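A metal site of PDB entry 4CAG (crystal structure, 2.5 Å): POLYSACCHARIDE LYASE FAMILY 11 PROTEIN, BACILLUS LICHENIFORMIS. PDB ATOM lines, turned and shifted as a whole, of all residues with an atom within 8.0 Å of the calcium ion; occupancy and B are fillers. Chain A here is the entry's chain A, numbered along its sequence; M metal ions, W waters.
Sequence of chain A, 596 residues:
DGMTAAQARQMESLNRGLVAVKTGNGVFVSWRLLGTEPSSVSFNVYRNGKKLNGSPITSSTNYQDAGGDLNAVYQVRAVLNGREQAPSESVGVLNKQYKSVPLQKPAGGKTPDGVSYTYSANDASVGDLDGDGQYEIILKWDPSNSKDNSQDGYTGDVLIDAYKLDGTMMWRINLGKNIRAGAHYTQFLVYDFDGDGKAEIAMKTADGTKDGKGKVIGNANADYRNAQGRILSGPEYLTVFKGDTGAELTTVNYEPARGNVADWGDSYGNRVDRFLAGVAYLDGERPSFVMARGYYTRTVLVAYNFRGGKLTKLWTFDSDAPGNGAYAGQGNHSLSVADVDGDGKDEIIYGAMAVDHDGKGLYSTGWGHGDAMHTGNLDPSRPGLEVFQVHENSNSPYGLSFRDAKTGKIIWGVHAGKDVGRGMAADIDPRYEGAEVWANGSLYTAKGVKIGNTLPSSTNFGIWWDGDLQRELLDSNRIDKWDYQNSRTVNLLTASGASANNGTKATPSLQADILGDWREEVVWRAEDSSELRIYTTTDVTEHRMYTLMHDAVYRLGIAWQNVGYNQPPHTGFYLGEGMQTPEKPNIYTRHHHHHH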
ATOM      1  N   LEU A 378     -17.962 -31.240  -5.773  1.00  0.00           N
ATOM      2  CA  LEU A 378     -17.101 -30.547  -4.834  1.00  0.00           C
ATOM      3  C   LEU A 378     -16.125 -31.527  -4.208  1.00  0.00           C
ATOM      4  O   LEU A 378     -14.936 -31.211  -4.019  1.00  0.00           O
ATOM      5  CB  LEU A 378     -17.976 -29.878  -3.783  1.00  0.00           C
ATOM      6  CG  LEU A 378     -18.425 -28.457  -4.150  1.00  0.00           C
ATOM      7  CD1 LEU A 378     -18.560 -28.215  -5.623  1.00  0.00           C
ATOM      8  CD2 LEU A 378     -19.732 -28.139  -3.434  1.00  0.00           C
ATOM      9  N   PRO A 380     -14.544 -34.814  -5.290  1.00  0.00           N
ATOM     10  CA  PRO A 380     -14.473 -35.742  -6.421  1.00  0.00           C
ATOM     11  C   PRO A 380     -14.419 -37.229  -5.985  1.00  0.00           C
ATOM     12  O   PRO A 380     -14.533 -38.074  -6.853  1.00  0.00           O
ATOM     13  CB  PRO A 380     -13.212 -35.320  -7.164  1.00  0.00           C
ATOM     14  CG  PRO A 380     -12.352 -34.596  -6.118  1.00  0.00           C
ATOM     15  CD  PRO A 380     -13.310 -34.026  -5.104  1.00  0.00           C
ATOM     16  N   ALA A 426     -14.529 -23.595  -3.772  1.00  0.00           N
ATOM     17  CA  ALA A 426     -13.512 -23.647  -4.816  1.00  0.00           C
ATOM     18  C   ALA A 426     -12.274 -24.391  -4.349  1.00  0.00           C
ATOM     19  O   ALA A 426     -11.944 -24.404  -3.157  1.00  0.00           O
ATOM     20  CB  ALA A 426     -13.123 -22.231  -5.229  1.00  0.00           C
ATOM     21  N   ASP A 427     -11.570 -24.979  -5.297  1.00  0.00           N
ATOM     22  CA  ASP A 427     -10.258 -25.537  -5.030  1.00  0.00           C
ATOM     23  C   ASP A 427      -9.249 -24.392  -4.953  1.00  0.00           C
ATOM     24  O   ASP A 427      -8.794 -23.866  -5.978  1.00  0.00           O
ATOM     25  CB  ASP A 427      -9.875 -26.547  -6.116  1.00  0.00           C
ATOM     26  CG  ASP A 427      -8.498 -27.175  -5.866  1.00  0.00           C
ATOM     27  OD1 ASP A 427      -7.978 -27.078  -4.727  1.00  0.00           O
ATOM     28  OD2 ASP A 427      -7.944 -27.767  -6.814  1.00  0.00           O
ATOM     29  N   ILE A 428      -8.915 -24.007  -3.721  1.00  0.00           N
ATOM     30  CA  ILE A 428      -7.918 -22.959  -3.491  1.00  0.00           C
ATOM     31  C   ILE A 428      -6.717 -23.560  -2.748  1.00  0.00           C
ATOM     32  O   ILE A 428      -5.691 -22.909  -2.586  1.00  0.00           O
ATOM     33  CB  ILE A 428      -8.517 -21.786  -2.690  1.00  0.00           C
ATOM     34  CG1 ILE A 428      -9.079 -22.282  -1.357  1.00  0.00           C
ATOM     35  CG2 ILE A 428      -9.646 -21.123  -3.507  1.00  0.00           C
ATOM     36  CD1 ILE A 428      -9.452 -21.171  -0.398  1.00  0.00           C
ATOM     37  N   ASP A 429      -6.873 -24.806  -2.306  1.00  0.00           N
ATOM     38  CA  ASP A 429      -5.834 -25.513  -1.550  1.00  0.00           C
ATOM     39  C   ASP A 429      -5.529 -26.851  -2.203  1.00  0.00           C
ATOM     40  O   ASP A 429      -6.347 -27.751  -2.119  1.00  0.00           O
ATOM     41  CB  ASP A 429      -6.257 -25.744  -0.085  1.00  0.00           C
ATOM     42  CG  ASP A 429      -5.048 -25.972   0.830  1.00  0.00           C
ATOM     43  OD1 ASP A 429      -4.032 -26.554   0.369  1.00  0.00           O
ATOM     44  OD2 ASP A 429      -5.080 -25.501   1.984  1.00  0.00           O
ATOM     45  N   PRO A 430      -4.334 -26.993  -2.816  1.00  0.00           N
ATOM     46  CA  PRO A 430      -3.990 -28.252  -3.490  1.00  0.00           C
ATOM     47  C   PRO A 430      -3.620 -29.362  -2.494  1.00  0.00           C
ATOM     48  O   PRO A 430      -3.570 -30.529  -2.879  1.00  0.00           O
ATOM     49  CB  PRO A 430      -2.769 -27.864  -4.334  1.00  0.00           C
ATOM     50  CG  PRO A 430      -2.111 -26.734  -3.570  1.00  0.00           C
ATOM     51  CD  PRO A 430      -3.222 -26.022  -2.838  1.00  0.00           C
ATOM     52  N   ARG A 431      -3.374 -29.023  -1.233  1.00  0.00           N
ATOM     53  CA  ARG A 431      -3.088 -30.058  -0.244  1.00  0.00           C
ATOM     54  C   ARG A 431      -4.284 -31.028  -0.046  1.00  0.00           C
ATOM     55  O   ARG A 431      -4.091 -32.117   0.504  1.00  0.00           O
ATOM     56  CB  ARG A 431      -2.691 -29.439   1.094  1.00  0.00           C
ATOM     57  CG  ARG A 431      -1.507 -28.495   1.009  1.00  0.00           C
ATOM     58  CD  ARG A 431      -1.204 -27.844   2.349  1.00  0.00           C
ATOM     59  NE  ARG A 431      -2.147 -26.775   2.707  1.00  0.00           N
ATOM     60  CZ  ARG A 431      -2.296 -26.284   3.947  1.00  0.00           C
ATOM     61  NH1 ARG A 431      -1.597 -26.780   4.966  1.00  0.00           N
ATOM     62  NH2 ARG A 431      -3.178 -25.314   4.168  1.00  0.00           N
ATOM     63  N   TYR A 432      -5.486 -30.623  -0.455  1.00  0.00           N
ATOM     64  CA  TYR A 432      -6.695 -31.428  -0.200  1.00  0.00           C
ATOM     65  C   TYR A 432      -7.467 -31.567  -1.464  1.00  0.00           C
ATOM     66  O   TYR A 432      -7.894 -30.577  -2.027  1.00  0.00           O
ATOM     67  CB  TYR A 432      -7.579 -30.803   0.861  1.00  0.00           C
ATOM     68  CG  TYR A 432      -6.779 -30.507   2.118  1.00  0.00           C
ATOM     69  CD1 TYR A 432      -6.242 -31.550   2.867  1.00  0.00           C
ATOM     70  CD2 TYR A 432      -6.512 -29.202   2.532  1.00  0.00           C
ATOM     71  CE1 TYR A 432      -5.490 -31.293   4.003  1.00  0.00           C
ATOM     72  CE2 TYR A 432      -5.751 -28.945   3.665  1.00  0.00           C
ATOM     73  CZ  TYR A 432      -5.242 -30.004   4.398  1.00  0.00           C
ATOM     74  OH  TYR A 432      -4.491 -29.790   5.540  1.00  0.00           O
ATOM     75  N   GLU A 433      -7.568 -32.797  -1.960  1.00  0.00           N
ATOM     76  CA  GLU A 433      -8.232 -33.041  -3.233  1.00  0.00           C
ATOM     77  C   GLU A 433      -9.700 -32.624  -3.128  1.00  0.00           C
ATOM     78  O   GLU A 433     -10.372 -32.929  -2.143  1.00  0.00           O
ATOM     79  CB  GLU A 433      -8.072 -34.506  -3.685  1.00  0.00           C
ATOM     80  CG  GLU A 433      -8.528 -34.731  -5.121  1.00  0.00           C
ATOM     81  CD  GLU A 433      -7.941 -35.974  -5.803  1.00  0.00           C
ATOM     82  OE1 GLU A 433      -6.824 -35.893  -6.400  1.00  0.00           O
ATOM     83  OE2 GLU A 433      -8.630 -37.001  -5.786  1.00  0.00           O
ATOM     84  N   GLY A 434     -10.162 -31.847  -4.094  1.00  0.00           N
ATOM     85  CA  GLY A 434     -11.524 -31.376  -4.085  1.00  0.00           C
ATOM     86  C   GLY A 434     -11.557 -29.902  -3.808  1.00  0.00           C
ATOM     87  O   GLY A 434     -10.514 -29.255  -3.715  1.00  0.00           O
ATOM     88  N   ALA A 435     -12.767 -29.367  -3.687  1.00  0.00           N
ATOM     89  CA  ALA A 435     -12.932 -27.939  -3.556  1.00  0.00           C
ATOM     90  C   ALA A 435     -12.946 -27.629  -2.075  1.00  0.00           C
ATOM     91  O   ALA A 435     -13.596 -28.362  -1.340  1.00  0.00           O
ATOM     92  CB  ALA A 435     -14.262 -27.522  -4.193  1.00  0.00           C
ATOM     93  N   GLU A 436     -12.268 -26.572  -1.643  1.00  0.00           N
ATOM     94  CA  GLU A 436     -12.445 -26.078  -0.277  1.00  0.00           C
ATOM     95  C   GLU A 436     -13.730 -25.237  -0.199  1.00  0.00           C
ATOM     96  O   GLU A 436     -14.222 -24.771  -1.231  1.00  0.00           O
ATOM     97  CB  GLU A 436     -11.232 -25.266   0.159  1.00  0.00           C
ATOM     98  CG  GLU A 436      -9.955 -26.103   0.431  1.00  0.00           C
ATOM     99  CD  GLU A 436      -9.446 -26.876  -0.810  1.00  0.00           C
ATOM    100  OE1 GLU A 436      -9.101 -26.284  -1.851  1.00  0.00           O
ATOM    101  OE2 GLU A 436      -9.394 -28.097  -0.730  1.00  0.00           O
ATOM    102  N   VAL A 437     -14.275 -25.038   0.997  1.00  0.00           N
ATOM    103  CA  VAL A 437     -15.442 -24.160   1.156  1.00  0.00           C
ATOM    104  C   VAL A 437     -15.208 -23.183   2.294  1.00  0.00           C
ATOM    105  O   VAL A 437     -14.394 -23.461   3.189  1.00  0.00           O
ATOM    106  CB  VAL A 437     -16.753 -24.937   1.447  1.00  0.00           C
ATOM    107  CG1 VAL A 437     -17.062 -25.900   0.278  1.00  0.00           C
ATOM    108  CG2 VAL A 437     -16.673 -25.692   2.788  1.00  0.00           C
ATOM    109  N   TYR A 444     -12.886 -24.603   5.223  1.00  0.00           N
ATOM    110  CA  TYR A 444     -12.969 -26.043   5.488  1.00  0.00           C
ATOM    111  C   TYR A 444     -12.545 -26.872   4.257  1.00  0.00           C
ATOM    112  O   TYR A 444     -12.652 -26.395   3.111  1.00  0.00           O
ATOM    113  CB  TYR A 444     -14.404 -26.438   5.908  1.00  0.00           C
ATOM    114  CG  TYR A 444     -14.995 -25.675   7.100  1.00  0.00           C
ATOM    115  CD1 TYR A 444     -15.561 -24.405   6.927  1.00  0.00           C
ATOM    116  CD2 TYR A 444     -14.999 -26.215   8.389  1.00  0.00           C
ATOM    117  CE1 TYR A 444     -16.092 -23.697   7.977  1.00  0.00           C
ATOM    118  CE2 TYR A 444     -15.540 -25.503   9.467  1.00  0.00           C
ATOM    119  CZ  TYR A 444     -16.092 -24.248   9.246  1.00  0.00           C
ATOM    120  OH  TYR A 444     -16.624 -23.526  10.261  1.00  0.00           O
ATOM    121  N   THR A 445     -12.085 -28.103   4.486  1.00  0.00           N
ATOM    122  CA  THR A 445     -11.916 -29.042   3.387  1.00  0.00           C
ATOM    123  C   THR A 445     -13.305 -29.501   2.915  1.00  0.00           C
ATOM    124  O   THR A 445     -14.325 -29.267   3.585  1.00  0.00           O
ATOM    125  CB  THR A 445     -11.126 -30.323   3.760  1.00  0.00           C
ATOM    126  OG1 THR A 445     -11.924 -31.173   4.601  1.00  0.00           O
ATOM    127  CG2 THR A 445      -9.827 -29.996   4.466  1.00  0.00           C
ATOM    128  N   ALA A 446     -13.353 -30.159   1.772  1.00  0.00           N
ATOM    129  CA  ALA A 446     -14.590 -30.742   1.325  1.00  0.00           C
ATOM    130  C   ALA A 446     -15.138 -31.791   2.346  1.00  0.00           C
ATOM    131  O   ALA A 446     -16.293 -32.219   2.235  1.00  0.00           O
ATOM    132  CB  ALA A 446     -14.390 -31.368  -0.047  1.00  0.00           C
ATOM    133  N   ILE A 451      -9.525 -25.713   8.110  1.00  0.00           N
ATOM    134  CA  ILE A 451      -8.177 -25.301   7.740  1.00  0.00           C
ATOM    135  C   ILE A 451      -7.794 -23.975   8.401  1.00  0.00           C
ATOM    136  O   ILE A 451      -8.592 -23.031   8.425  1.00  0.00           O
ATOM    137  CB  ILE A 451      -8.102 -25.162   6.214  1.00  0.00           C
ATOM    138  CG1 ILE A 451      -8.512 -26.468   5.536  1.00  0.00           C
ATOM    139  CG2 ILE A 451      -6.696 -24.782   5.777  1.00  0.00           C
ATOM    140  CD1 ILE A 451      -8.945 -26.297   4.133  1.00  0.00           C
ATOM    141  N   LEU A 469      -4.737 -25.153 -11.672  1.00  0.00           N
ATOM    142  CA  LEU A 469      -6.036 -25.817 -11.622  1.00  0.00           C
ATOM    143  C   LEU A 469      -6.823 -25.416 -10.416  1.00  0.00           C
ATOM    144  O   LEU A 469      -7.991 -25.800 -10.282  1.00  0.00           O
ATOM    145  CB  LEU A 469      -5.906 -27.337 -11.660  1.00  0.00           C
ATOM    146  CG  LEU A 469      -5.424 -27.871 -13.007  1.00  0.00           C
ATOM    147  CD1 LEU A 469      -5.078 -29.335 -12.850  1.00  0.00           C
ATOM    148  CD2 LEU A 469      -6.446 -27.635 -14.135  1.00  0.00           C
ATOM    149  N   GLN A 470      -6.197 -24.669  -9.510  1.00  0.00           N
ATOM    150  CA  GLN A 470      -6.973 -24.057  -8.446  1.00  0.00           C
ATOM    151  C   GLN A 470      -7.844 -22.985  -9.090  1.00  0.00           C
ATOM    152  O   GLN A 470      -7.611 -22.585 -10.232  1.00  0.00           O
ATOM    153  CB  GLN A 470      -6.091 -23.453  -7.350  1.00  0.00           C
ATOM    154  CG  GLN A 470      -5.626 -24.456  -6.289  1.00  0.00           C
ATOM    155  CD  GLN A 470      -4.555 -25.400  -6.865  1.00  0.00           C
ATOM    156  OE1 GLN A 470      -3.383 -25.014  -7.016  1.00  0.00           O
ATOM    157  NE2 GLN A 470      -4.972 -26.630  -7.232  1.00  0.00           N
ATOM    158  N   TYR A 574     -15.444 -32.486 -12.126  1.00  0.00           N
ATOM    159  CA  TYR A 574     -14.529 -31.957 -11.159  1.00  0.00           C
ATOM    160  C   TYR A 574     -13.359 -31.246 -11.874  1.00  0.00           C
ATOM    161  O   TYR A 574     -12.608 -31.874 -12.633  1.00  0.00           O
ATOM    162  CB  TYR A 574     -14.025 -33.042 -10.238  1.00  0.00           C
ATOM    163  CG  TYR A 574     -12.866 -32.560  -9.416  1.00  0.00           C
ATOM    164  CD1 TYR A 574     -13.047 -31.611  -8.409  1.00  0.00           C
ATOM    165  CD2 TYR A 574     -11.586 -33.041  -9.643  1.00  0.00           C
ATOM    166  CE1 TYR A 574     -11.996 -31.152  -7.669  1.00  0.00           C
ATOM    167  CE2 TYR A 574     -10.510 -32.594  -8.892  1.00  0.00           C
ATOM    168  CZ  TYR A 574     -10.719 -31.661  -7.901  1.00  0.00           C
ATOM    169  OH  TYR A 574      -9.625 -31.207  -7.162  1.00  0.00           O
ATOM    170  N   GLY A 576     -10.097 -29.219 -10.909  1.00  0.00           N
ATOM    171  CA  GLY A 576      -9.146 -28.921  -9.845  1.00  0.00           C
ATOM    172  C   GLY A 576      -7.973 -29.900  -9.805  1.00  0.00           C
ATOM    173  O   GLY A 576      -7.886 -30.818 -10.640  1.00  0.00           O
ATOM    174  N   GLU A 577      -7.092 -29.695  -8.828  1.00  0.00           N
ATOM    175  CA  GLU A 577      -5.908 -30.550  -8.634  1.00  0.00           C
ATOM    176  C   GLU A 577      -6.317 -32.021  -8.549  1.00  0.00           C
ATOM    177  O   GLU A 577      -7.193 -32.392  -7.782  1.00  0.00           O
ATOM    178  CB  GLU A 577      -5.186 -30.128  -7.343  1.00  0.00           C
ATOM    179  CG  GLU A 577      -3.643 -30.328  -7.336  1.00  0.00           C
ATOM    180  CD  GLU A 577      -2.848 -29.385  -8.255  1.00  0.00           C
ATOM    181  OE1 GLU A 577      -3.214 -28.180  -8.400  1.00  0.00           O
ATOM    182  OE2 GLU A 577      -1.828 -29.860  -8.832  1.00  0.00           O
HETATM  183 CA    CA M   1      -8.486 -28.400  -2.766  1.00  0.00          CA
HETATM  184  O   HOH W   1      -7.682 -29.635  -4.579  1.00  0.00           O
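N of Glu 577 sits at hydrogen-bond distance from OD2 of Asp 427. OH of Tyr 574 is in hydrogen-bond range of N of Gly 434, 3.2 Å away. The backbone NH (N) of Glu 436 is in hydrogen-bond range of the backbone carbonyl oxygen (O) of Ala 426 (2.7 Å). The side-chain carboxylate of Glu 436 sits close to the backbone NH of Ile 428 (3.0 Å). The side-chain carboxylate (OD2) of Asp 427 lies within hydrogen-bond range of the side-chain amide nitrogen (NE2) of Gln 470 (3.2 Å). The side-chain carboxylate (OD2) of Asp 429 lies within salt-bridge range of the guanidinium group (NH2) of Arg 431, at 2.9 Å.
Within 4 Å of the calcium ion: Asp 427, Asp 429, Tyr 432, Gly 434 and Glu 436. The nearest printed residue that does not touch the calcium ion is Pro 430 (4.4 Å).
The calcium ion is bound by OE2 of Glu 436. The calcium ion is bound by the backbone carbonyl oxygen (O) of Asp 429, at 2.3 Å. Water W1 binds the calcium ion (2.3 Å). The calcium ion is bound by O of Tyr 432, at 2.4 Å. OE1 of Glu 436 binds the calcium ion, at 2.4 Å. The calcium ion is bound by the backbone carbonyl oxygen (O) of Gly 434 (2.4 Å). OD1 of Asp 427 is bound to the calcium ion (2.4 Å). The calcium ion has seven donor atoms within binding distance.
Water W1 bridges OD2 of Asp 427 (2.9 Å) and N of Gly 434 (3.4 Å).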
